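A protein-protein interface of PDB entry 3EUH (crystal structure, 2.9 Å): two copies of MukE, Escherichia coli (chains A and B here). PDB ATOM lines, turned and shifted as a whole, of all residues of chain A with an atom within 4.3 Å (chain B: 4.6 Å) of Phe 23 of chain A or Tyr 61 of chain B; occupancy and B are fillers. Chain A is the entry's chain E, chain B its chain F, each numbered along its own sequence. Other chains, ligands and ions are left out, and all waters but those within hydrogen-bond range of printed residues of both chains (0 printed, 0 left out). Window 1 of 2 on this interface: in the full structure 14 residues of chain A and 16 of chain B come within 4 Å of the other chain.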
ATOM      1  N   ALA A  17      35.332  -8.677  27.503  1.00  0.00           N
ATOM      2  CA  ALA A  17      34.326  -8.980  26.501  1.00  0.00           C
ATOM      3  C   ALA A  17      33.221  -9.846  27.095  1.00  0.00           C
ATOM      4  O   ALA A  17      32.074  -9.406  27.200  1.00  0.00           O
ATOM      5  CB  ALA A  17      34.966  -9.675  25.300  1.00  0.00           C
ATOM      6  N   LEU A  18      33.566 -11.071  27.488  1.00  0.00           N
ATOM      7  CA  LEU A  18      32.587 -11.984  28.059  1.00  0.00           C
ATOM      8  C   LEU A  18      31.670 -11.326  29.083  1.00  0.00           C
ATOM      9  O   LEU A  18      30.602 -11.835  29.365  1.00  0.00           O
ATOM     10  CB  LEU A  18      33.297 -13.177  28.705  1.00  0.00           C
ATOM     11  CG  LEU A  18      33.176 -14.538  28.006  1.00  0.00           C
ATOM     12  CD1 LEU A  18      33.631 -14.443  26.558  1.00  0.00           C
ATOM     13  CD2 LEU A  18      34.016 -15.558  28.752  1.00  0.00           C
ATOM     14  N   ASN A  20      30.947  -7.864  28.893  1.00  0.00           N
ATOM     15  CA  ASN A  20      30.253  -6.781  28.226  1.00  0.00           C
ATOM     16  C   ASN A  20      28.763  -7.150  28.125  1.00  0.00           C
ATOM     17  O   ASN A  20      28.412  -8.313  27.904  1.00  0.00           O
ATOM     18  CB  ASN A  20      30.870  -6.572  26.841  1.00  0.00           C
ATOM     19  CG  ASN A  20      30.235  -5.430  26.083  1.00  0.00           C
ATOM     20  OD1 ASN A  20      30.927  -4.539  25.581  1.00  0.00           O
ATOM     21  ND2 ASN A  20      28.914  -5.455  25.979  1.00  0.00           N
ATOM     22  N   PRO A  21      27.868  -6.165  28.312  1.00  0.00           N
ATOM     23  CA  PRO A  21      26.405  -6.332  28.249  1.00  0.00           C
ATOM     24  C   PRO A  21      25.867  -6.909  26.927  1.00  0.00           C
ATOM     25  O   PRO A  21      24.781  -7.487  26.893  1.00  0.00           O
ATOM     26  CB  PRO A  21      25.890  -4.912  28.482  1.00  0.00           C
ATOM     27  CG  PRO A  21      26.937  -4.323  29.344  1.00  0.00           C
ATOM     28  CD  PRO A  21      28.209  -4.786  28.701  1.00  0.00           C
ATOM     29  N   LEU A  22      26.628  -6.750  25.851  1.00  0.00           N
ATOM     30  CA  LEU A  22      26.201  -7.221  24.538  1.00  0.00           C
ATOM     31  C   LEU A  22      26.398  -8.718  24.231  1.00  0.00           C
ATOM     32  O   LEU A  22      25.730  -9.290  23.350  1.00  0.00           O
ATOM     33  CB  LEU A  22      26.919  -6.401  23.467  1.00  0.00           C
ATOM     34  CG  LEU A  22      26.529  -4.927  23.343  1.00  0.00           C
ATOM     35  CD1 LEU A  22      27.158  -4.330  22.088  1.00  0.00           C
ATOM     36  CD2 LEU A  22      25.010  -4.811  23.266  1.00  0.00           C
ATOM     37  N   PHE A  23      27.293  -9.345  24.990  1.00  0.00           N
ATOM     38  CA  PHE A  23      27.676 -10.729  24.784  1.00  0.00           C
ATOM     39  C   PHE A  23      26.631 -11.819  24.841  1.00  0.00           C
ATOM     40  O   PHE A  23      26.405 -12.516  23.862  1.00  0.00           O
ATOM     41  CB  PHE A  23      28.812 -11.079  25.733  1.00  0.00           C
ATOM     42  CG  PHE A  23      29.364 -12.449  25.530  1.00  0.00           C
ATOM     43  CD1 PHE A  23      30.212 -12.724  24.457  1.00  0.00           C
ATOM     44  CD2 PHE A  23      29.014 -13.480  26.394  1.00  0.00           C
ATOM     45  CE1 PHE A  23      30.707 -14.015  24.247  1.00  0.00           C
ATOM     46  CE2 PHE A  23      29.498 -14.762  26.196  1.00  0.00           C
ATOM     47  CZ  PHE A  23      30.351 -15.035  25.115  1.00  0.00           C
ATOM     48  N   PRO A  24      25.980 -11.999  25.985  1.00  0.00           N
ATOM     49  CA  PRO A  24      24.990 -13.078  25.988  1.00  0.00           C
ATOM     50  C   PRO A  24      24.013 -13.092  24.824  1.00  0.00           C
ATOM     51  O   PRO A  24      23.756 -14.143  24.247  1.00  0.00           O
ATOM     52  CB  PRO A  24      24.319 -12.945  27.353  1.00  0.00           C
ATOM     53  CG  PRO A  24      24.662 -11.558  27.804  1.00  0.00           C
ATOM     54  CD  PRO A  24      26.015 -11.281  27.265  1.00  0.00           C
ATOM     55  N   ALA A  25      23.478 -11.941  24.450  1.00  0.00           N
ATOM     56  CA  ALA A  25      22.538 -11.928  23.334  1.00  0.00           C
ATOM     57  C   ALA A  25      23.277 -12.251  22.034  1.00  0.00           C
ATOM     58  O   ALA A  25      22.809 -13.063  21.236  1.00  0.00           O
ATOM     59  CB  ALA A  25      21.829 -10.570  23.242  1.00  0.00           C
ATOM     60  N   LEU A  26      24.441 -11.635  21.837  1.00  0.00           N
ATOM     61  CA  LEU A  26      25.244 -11.872  20.638  1.00  0.00           C
ATOM     62  C   LEU A  26      25.641 -13.350  20.522  1.00  0.00           C
ATOM     63  O   LEU A  26      25.496 -13.967  19.458  1.00  0.00           O
ATOM     64  CB  LEU A  26      26.510 -11.030  20.677  1.00  0.00           C
ATOM     65  CG  LEU A  26      26.754 -10.161  19.454  1.00  0.00           C
ATOM     66  CD1 LEU A  26      28.221  -9.730  19.510  1.00  0.00           C
ATOM     67  CD2 LEU A  26      26.427 -10.917  18.148  1.00  0.00           C
ATOM     68  N   ASP A  27      26.155 -13.893  21.623  1.00  0.00           N
ATOM     69  CA  ASP A  27      26.567 -15.278  21.705  1.00  0.00           C
ATOM     70  C   ASP A  27      25.369 -16.109  21.290  1.00  0.00           C
ATOM     71  O   ASP A  27      25.452 -16.932  20.384  1.00  0.00           O
ATOM     72  CB  ASP A  27      26.997 -15.616  23.143  1.00  0.00           C
ATOM     73  CG  ASP A  27      27.441 -17.070  23.308  1.00  0.00           C
ATOM     74  OD1 ASP A  27      28.227 -17.550  22.456  1.00  0.00           O
ATOM     75  OD2 ASP A  27      27.008 -17.728  24.287  1.00  0.00           O
ATOM     76  N   LEU A  54      37.369 -13.313  21.318  1.00  0.00           N
ATOM     77  CA  LEU A  54      36.174 -14.102  21.087  1.00  0.00           C
ATOM     78  C   LEU A  54      36.541 -15.254  20.144  1.00  0.00           C
ATOM     79  O   LEU A  54      35.884 -16.295  20.122  1.00  0.00           O
ATOM     80  CB  LEU A  54      35.080 -13.213  20.502  1.00  0.00           C
ATOM     81  CG  LEU A  54      34.418 -12.361  21.588  1.00  0.00           C
ATOM     82  CD1 LEU A  54      33.582 -11.256  20.985  1.00  0.00           C
ATOM     83  CD2 LEU A  54      33.547 -13.258  22.444  1.00  0.00           C
ATOM     84  N   PHE A  57      37.722 -17.776  22.465  1.00  0.00           N
ATOM     85  CA  PHE A  57      36.555 -18.338  23.135  1.00  0.00           C
ATOM     86  C   PHE A  57      35.766 -19.382  22.339  1.00  0.00           C
ATOM     87  O   PHE A  57      35.489 -20.479  22.832  1.00  0.00           O
ATOM     88  CB  PHE A  57      35.625 -17.201  23.570  1.00  0.00           C
ATOM     89  CG  PHE A  57      34.348 -17.673  24.180  1.00  0.00           C
ATOM     90  CD1 PHE A  57      34.339 -18.258  25.436  1.00  0.00           C
ATOM     91  CD2 PHE A  57      33.159 -17.605  23.461  1.00  0.00           C
ATOM     92  CE1 PHE A  57      33.164 -18.778  25.974  1.00  0.00           C
ATOM     93  CE2 PHE A  57      31.982 -18.124  23.989  1.00  0.00           C
ATOM     94  CZ  PHE A  57      31.989 -18.716  25.251  1.00  0.00           C
ATOM     95  N   TYR A  58      35.393 -19.037  21.114  1.00  0.00           N
ATOM     96  CA  TYR A  58      34.624 -19.955  20.292  1.00  0.00           C
ATOM     97  C   TYR A  58      35.424 -21.168  19.829  1.00  0.00           C
ATOM     98  O   TYR A  58      34.874 -22.263  19.654  1.00  0.00           O
ATOM     99  CB  TYR A  58      34.013 -19.196  19.110  1.00  0.00           C
ATOM    100  CG  TYR A  58      32.838 -18.355  19.544  1.00  0.00           C
ATOM    101  CD1 TYR A  58      32.902 -16.968  19.538  1.00  0.00           C
ATOM    102  CD2 TYR A  58      31.690 -18.959  20.043  1.00  0.00           C
ATOM    103  CE1 TYR A  58      31.860 -16.207  20.027  1.00  0.00           C
ATOM    104  CE2 TYR A  58      30.640 -18.214  20.537  1.00  0.00           C
ATOM    105  CZ  TYR A  58      30.727 -16.835  20.532  1.00  0.00           C
ATOM    106  OH  TYR A  58      29.693 -16.090  21.066  1.00  0.00           O
ATOM    107  N   ARG B  31      22.499 -25.684  27.791  1.00  0.00           N
ATOM    108  CA  ARG B  31      21.694 -24.803  26.953  1.00  0.00           C
ATOM    109  C   ARG B  31      20.739 -25.557  26.062  1.00  0.00           C
ATOM    110  O   ARG B  31      19.805 -24.975  25.501  1.00  0.00           O
ATOM    111  CB  ARG B  31      22.589 -23.904  26.100  1.00  0.00           C
ATOM    112  CG  ARG B  31      23.503 -23.035  26.923  1.00  0.00           C
ATOM    113  CD  ARG B  31      24.148 -21.940  26.101  1.00  0.00           C
ATOM    114  NE  ARG B  31      25.206 -21.285  26.860  1.00  0.00           N
ATOM    115  CZ  ARG B  31      25.793 -20.150  26.504  1.00  0.00           C
ATOM    116  NH1 ARG B  31      25.424 -19.528  25.394  1.00  0.00           N
ATOM    117  NH2 ARG B  31      26.762 -19.638  27.253  1.00  0.00           N
ATOM    118  N   PHE B  57      26.388 -16.539  35.930  1.00  0.00           N
ATOM    119  CA  PHE B  57      26.640 -16.530  34.497  1.00  0.00           C
ATOM    120  C   PHE B  57      25.353 -16.671  33.715  1.00  0.00           C
ATOM    121  O   PHE B  57      24.981 -15.787  32.947  1.00  0.00           O
ATOM    122  CB  PHE B  57      27.585 -17.666  34.111  1.00  0.00           C
ATOM    123  CG  PHE B  57      27.916 -17.714  32.641  1.00  0.00           C
ATOM    124  CD1 PHE B  57      28.618 -16.673  32.029  1.00  0.00           C
ATOM    125  CD2 PHE B  57      27.526 -18.809  31.862  1.00  0.00           C
ATOM    126  CE1 PHE B  57      28.930 -16.722  30.663  1.00  0.00           C
ATOM    127  CE2 PHE B  57      27.833 -18.867  30.492  1.00  0.00           C
ATOM    128  CZ  PHE B  57      28.535 -17.819  29.894  1.00  0.00           C
ATOM    129  N   TYR B  58      24.664 -17.783  33.915  1.00  0.00           N
ATOM    130  CA  TYR B  58      23.430 -18.003  33.193  1.00  0.00           C
ATOM    131  C   TYR B  58      22.335 -16.994  33.508  1.00  0.00           C
ATOM    132  O   TYR B  58      21.379 -16.847  32.755  1.00  0.00           O
ATOM    133  CB  TYR B  58      22.956 -19.439  33.416  1.00  0.00           C
ATOM    134  CG  TYR B  58      23.890 -20.439  32.783  1.00  0.00           C
ATOM    135  CD1 TYR B  58      24.655 -21.304  33.562  1.00  0.00           C
ATOM    136  CD2 TYR B  58      24.046 -20.486  31.398  1.00  0.00           C
ATOM    137  CE1 TYR B  58      25.557 -22.190  32.979  1.00  0.00           C
ATOM    138  CE2 TYR B  58      24.944 -21.368  30.804  1.00  0.00           C
ATOM    139  CZ  TYR B  58      25.695 -22.213  31.598  1.00  0.00           C
ATOM    140  OH  TYR B  58      26.585 -23.067  31.003  1.00  0.00           O
ATOM    141  N   ALA B  59      22.472 -16.289  34.619  1.00  0.00           N
ATOM    142  CA  ALA B  59      21.483 -15.275  34.970  1.00  0.00           C
ATOM    143  C   ALA B  59      21.538 -14.123  33.945  1.00  0.00           C
ATOM    144  O   ALA B  59      20.536 -13.442  33.679  1.00  0.00           O
ATOM    145  CB  ALA B  59      21.765 -14.750  36.358  1.00  0.00           C
ATOM    146  N   ARG B  60      22.722 -13.910  33.377  1.00  0.00           N
ATOM    147  CA  ARG B  60      22.926 -12.865  32.396  1.00  0.00           C
ATOM    148  C   ARG B  60      22.091 -13.214  31.171  1.00  0.00           C
ATOM    149  O   ARG B  60      21.795 -12.364  30.342  1.00  0.00           O
ATOM    150  CB  ARG B  60      24.414 -12.790  32.037  1.00  0.00           C
ATOM    151  CG  ARG B  60      25.123 -11.571  32.571  1.00  0.00           C
ATOM    152  CD  ARG B  60      26.539 -11.859  33.030  1.00  0.00           C
ATOM    153  NE  ARG B  60      27.553 -11.780  31.982  1.00  0.00           N
ATOM    154  CZ  ARG B  60      27.629 -10.808  31.083  1.00  0.00           C
ATOM    155  NH1 ARG B  60      26.746  -9.818  31.080  1.00  0.00           N
ATOM    156  NH2 ARG B  60      28.609 -10.811  30.193  1.00  0.00           N
ATOM    157  N   TYR B  61      21.701 -14.476  31.071  1.00  0.00           N
ATOM    158  CA  TYR B  61      20.906 -14.934  29.944  1.00  0.00           C
ATOM    159  C   TYR B  61      19.456 -15.079  30.336  1.00  0.00           C
ATOM    160  O   TYR B  61      18.667 -15.599  29.563  1.00  0.00           O
ATOM    161  CB  TYR B  61      21.394 -16.295  29.440  1.00  0.00           C
ATOM    162  CG  TYR B  61      22.761 -16.298  28.808  1.00  0.00           C
ATOM    163  CD1 TYR B  61      23.913 -16.214  29.584  1.00  0.00           C
ATOM    164  CD2 TYR B  61      22.902 -16.375  27.424  1.00  0.00           C
ATOM    165  CE1 TYR B  61      25.171 -16.203  29.001  1.00  0.00           C
ATOM    166  CE2 TYR B  61      24.155 -16.361  26.830  1.00  0.00           C
ATOM    167  CZ  TYR B  61      25.281 -16.271  27.628  1.00  0.00           C
ATOM    168  OH  TYR B  61      26.517 -16.204  27.042  1.00  0.00           O
ATOM    169  N   ASN B  62      19.103 -14.628  31.534  1.00  0.00           N
ATOM    170  CA  ASN B  62      17.725 -14.741  32.015  1.00  0.00           C
ATOM    171  C   ASN B  62      17.291 -16.190  32.046  1.00  0.00           C
ATOM    172  O   ASN B  62      16.189 -16.544  31.637  1.00  0.00           O
ATOM    173  CB  ASN B  62      16.769 -13.960  31.128  1.00  0.00           C
ATOM    174  CG  ASN B  62      17.057 -12.499  31.141  1.00  0.00           C
ATOM    175  OD1 ASN B  62      17.424 -11.942  32.171  1.00  0.00           O
ATOM    176  ND2 ASN B  62      16.877 -11.852  29.998  1.00  0.00           N
ATOM    177  N   VAL B  63      18.188 -17.020  32.545  1.00  0.00           N
ATOM    178  CA  VAL B  63      17.979 -18.446  32.671  1.00  0.00           C
ATOM    179  C   VAL B  63      18.451 -18.736  34.095  1.00  0.00           C
ATOM    180  O   VAL B  63      19.383 -18.087  34.569  1.00  0.00           O
ATOM    181  CB  VAL B  63      18.879 -19.187  31.644  1.00  0.00           C
ATOM    182  CG1 VAL B  63      19.035 -20.634  32.018  1.00  0.00           C
ATOM    183  CG2 VAL B  63      18.292 -19.054  30.249  1.00  0.00           C
ATOM    184  N   THR B  81      13.962 -15.043  28.608  1.00  0.00           N
ATOM    185  CA  THR B  81      15.180 -15.719  28.183  1.00  0.00           C
ATOM    186  C   THR B  81      15.910 -15.159  26.966  1.00  0.00           C
ATOM    187  O   THR B  81      15.312 -14.602  26.051  1.00  0.00           O
ATOM    188  CB  THR B  81      14.942 -17.223  27.939  1.00  0.00           C
ATOM    189  OG1 THR B  81      16.189 -17.845  27.587  1.00  0.00           O
ATOM    190  CG2 THR B  81      13.940 -17.435  26.812  1.00  0.00           C
ATOM    191  N   LEU B  82      17.226 -15.342  26.987  1.00  0.00           N
ATOM    192  CA  LEU B  82      18.130 -14.899  25.939  1.00  0.00           C
ATOM    193  C   LEU B  82      18.651 -16.108  25.166  1.00  0.00           C
ATOM    194  O   LEU B  82      19.444 -15.966  24.235  1.00  0.00           O
ATOM    195  CB  LEU B  82      19.301 -14.146  26.565  1.00  0.00           C
ATOM    196  CG  LEU B  82      19.421 -12.697  26.116  1.00  0.00           C
ATOM    197  CD1 LEU B  82      18.099 -11.989  26.323  1.00  0.00           C
ATOM    198  CD2 LEU B  82      20.557 -12.019  26.870  1.00  0.00           C
ATOM    199  N   ILE B  83      18.211 -17.297  25.580  1.00  0.00           N
ATOM    200  CA  ILE B  83      18.580 -18.561  24.946  1.00  0.00           C
ATOM    201  C   ILE B  83      17.294 -19.118  24.317  1.00  0.00           C
ATOM    202  O   ILE B  83      16.297 -19.274  25.016  1.00  0.00           O
ATOM    203  CB  ILE B  83      19.100 -19.559  26.002  1.00  0.00           C
ATOM    204  CG1 ILE B  83      20.469 -19.114  26.525  1.00  0.00           C
ATOM    205  CG2 ILE B  83      19.171 -20.948  25.411  1.00  0.00           C
ATOM    206  CD1 ILE B  83      20.929 -19.850  27.780  1.00  0.00           C
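ND2 of Asn 20 of chain A lies close to N of Leu 22 of chain A, 2.6 Å away. The backbone carbonyl oxygen of Tyr 61 of chain B lies within hydrogen-bond range of the backbone NH of Leu 82 of chain B (3.0 Å). The side-chain carboxylate (OD1) of Asp 27 of chain A sits at hydrogen-bond distance from the side-chain hydroxyl (OH) of Tyr 58 of chain A, at 2.5 Å. The guanidinium group (NH2) of Arg 31 of chain B is in hydrogen-bond range of the side-chain hydroxyl (OH) of Tyr 61 of chain B.
2 positions are printed for both chains. Of the 9 pairs that touch across the chains among the printed residues, none has its exchanged pair printed and touching as well.
Printed residues of chain B within 4 Å of Leu 18 of chain A: Arg 60 (2.4 Å). Of the printed residues of chain B, Asn 20 of chain A touches Arg 60. Of chain B, only Tyr 61 comes within 4 Å of Phe 23 of chain A. Printed residues of chain B within 4 Å of Pro 24 of chain A: Arg 60 (3.9 Å), Tyr 61 (3.4 Å) and Leu 82 (3.9 Å). Of the printed residues of chain B, Ala 25 of chain A touches Leu 82. Printed residues of chain B within 4 Å of Asp 27 of chain A: Arg 31 and Tyr 61. Phe 57 of chain A touches none of the printed residues of chain B. Ile 83 of chain B touches none of the printed residues of chain A. The nearest printed residue of chain A that does not touch Tyr 61 of chain B is Ala 25 of chain A (5.1 Å). The nearest printed residue of chain B that does not touch Asn 20 of chain A is Tyr 61 of chain B (8.2 Å).
Tyr 61 of chain B touches Phe 23 of chain A (OH to CE2, 3.4 Å). Arg 60 of chain B touches Pro 24 of chain A. Pro 24 of chain A touches Tyr 61 of chain B. CD2 of Leu 82 of chain B touches CB of Pro 24 of chain A, 3.9 Å away. Leu 82 of chain B touches Ala 25 of chain A (CD2 to N, 3.8 Å).
The side-chain carboxylate (OD2) of Asp 27 of chain A is in hydrogen-bond range of the side-chain hydroxyl (OH) of Tyr 61 of chain B (3.2 Å). The guanidinium group of Arg 31 of chain B lies within salt-bridge range of the side-chain carboxylate of Asp 27 of chain A (2.6 Å). The backbone carbonyl oxygen of Asn 20 of chain A sits at hydrogen-bond distance from the guanidinium group of Arg 60 of chain B (3.4 Å). The backbone carbonyl oxygen of Leu 18 of chain A sits close to the guanidinium group of Arg 60 of chain B (2.4 Å).
Of the 11 printed residues of chain B, 4 touch a printed residue of chain A. Hydrophobic or aromatic side chains of chain B that line the printed part of chain A: Tyr 61 and Leu 82. Of the 13 printed residues of chain A, 6 touch a printed residue of chain B. Printed residues of chain A that touch a printed residue of chain B: Leu 18, Asn 20, Phe 23, Pro 24, Ala 25 and Asp 27. Hydrophobic or aromatic side chains of chain A that line the printed part of chain B: Phe 23 and Pro 24. Among the printed residues, Asp or Glu carboxylates within 4 Å of a Lys or Arg side-chain nitrogen of the other chain: Asp 27 of chain A with Arg 31 of chain B (2.6 Å).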
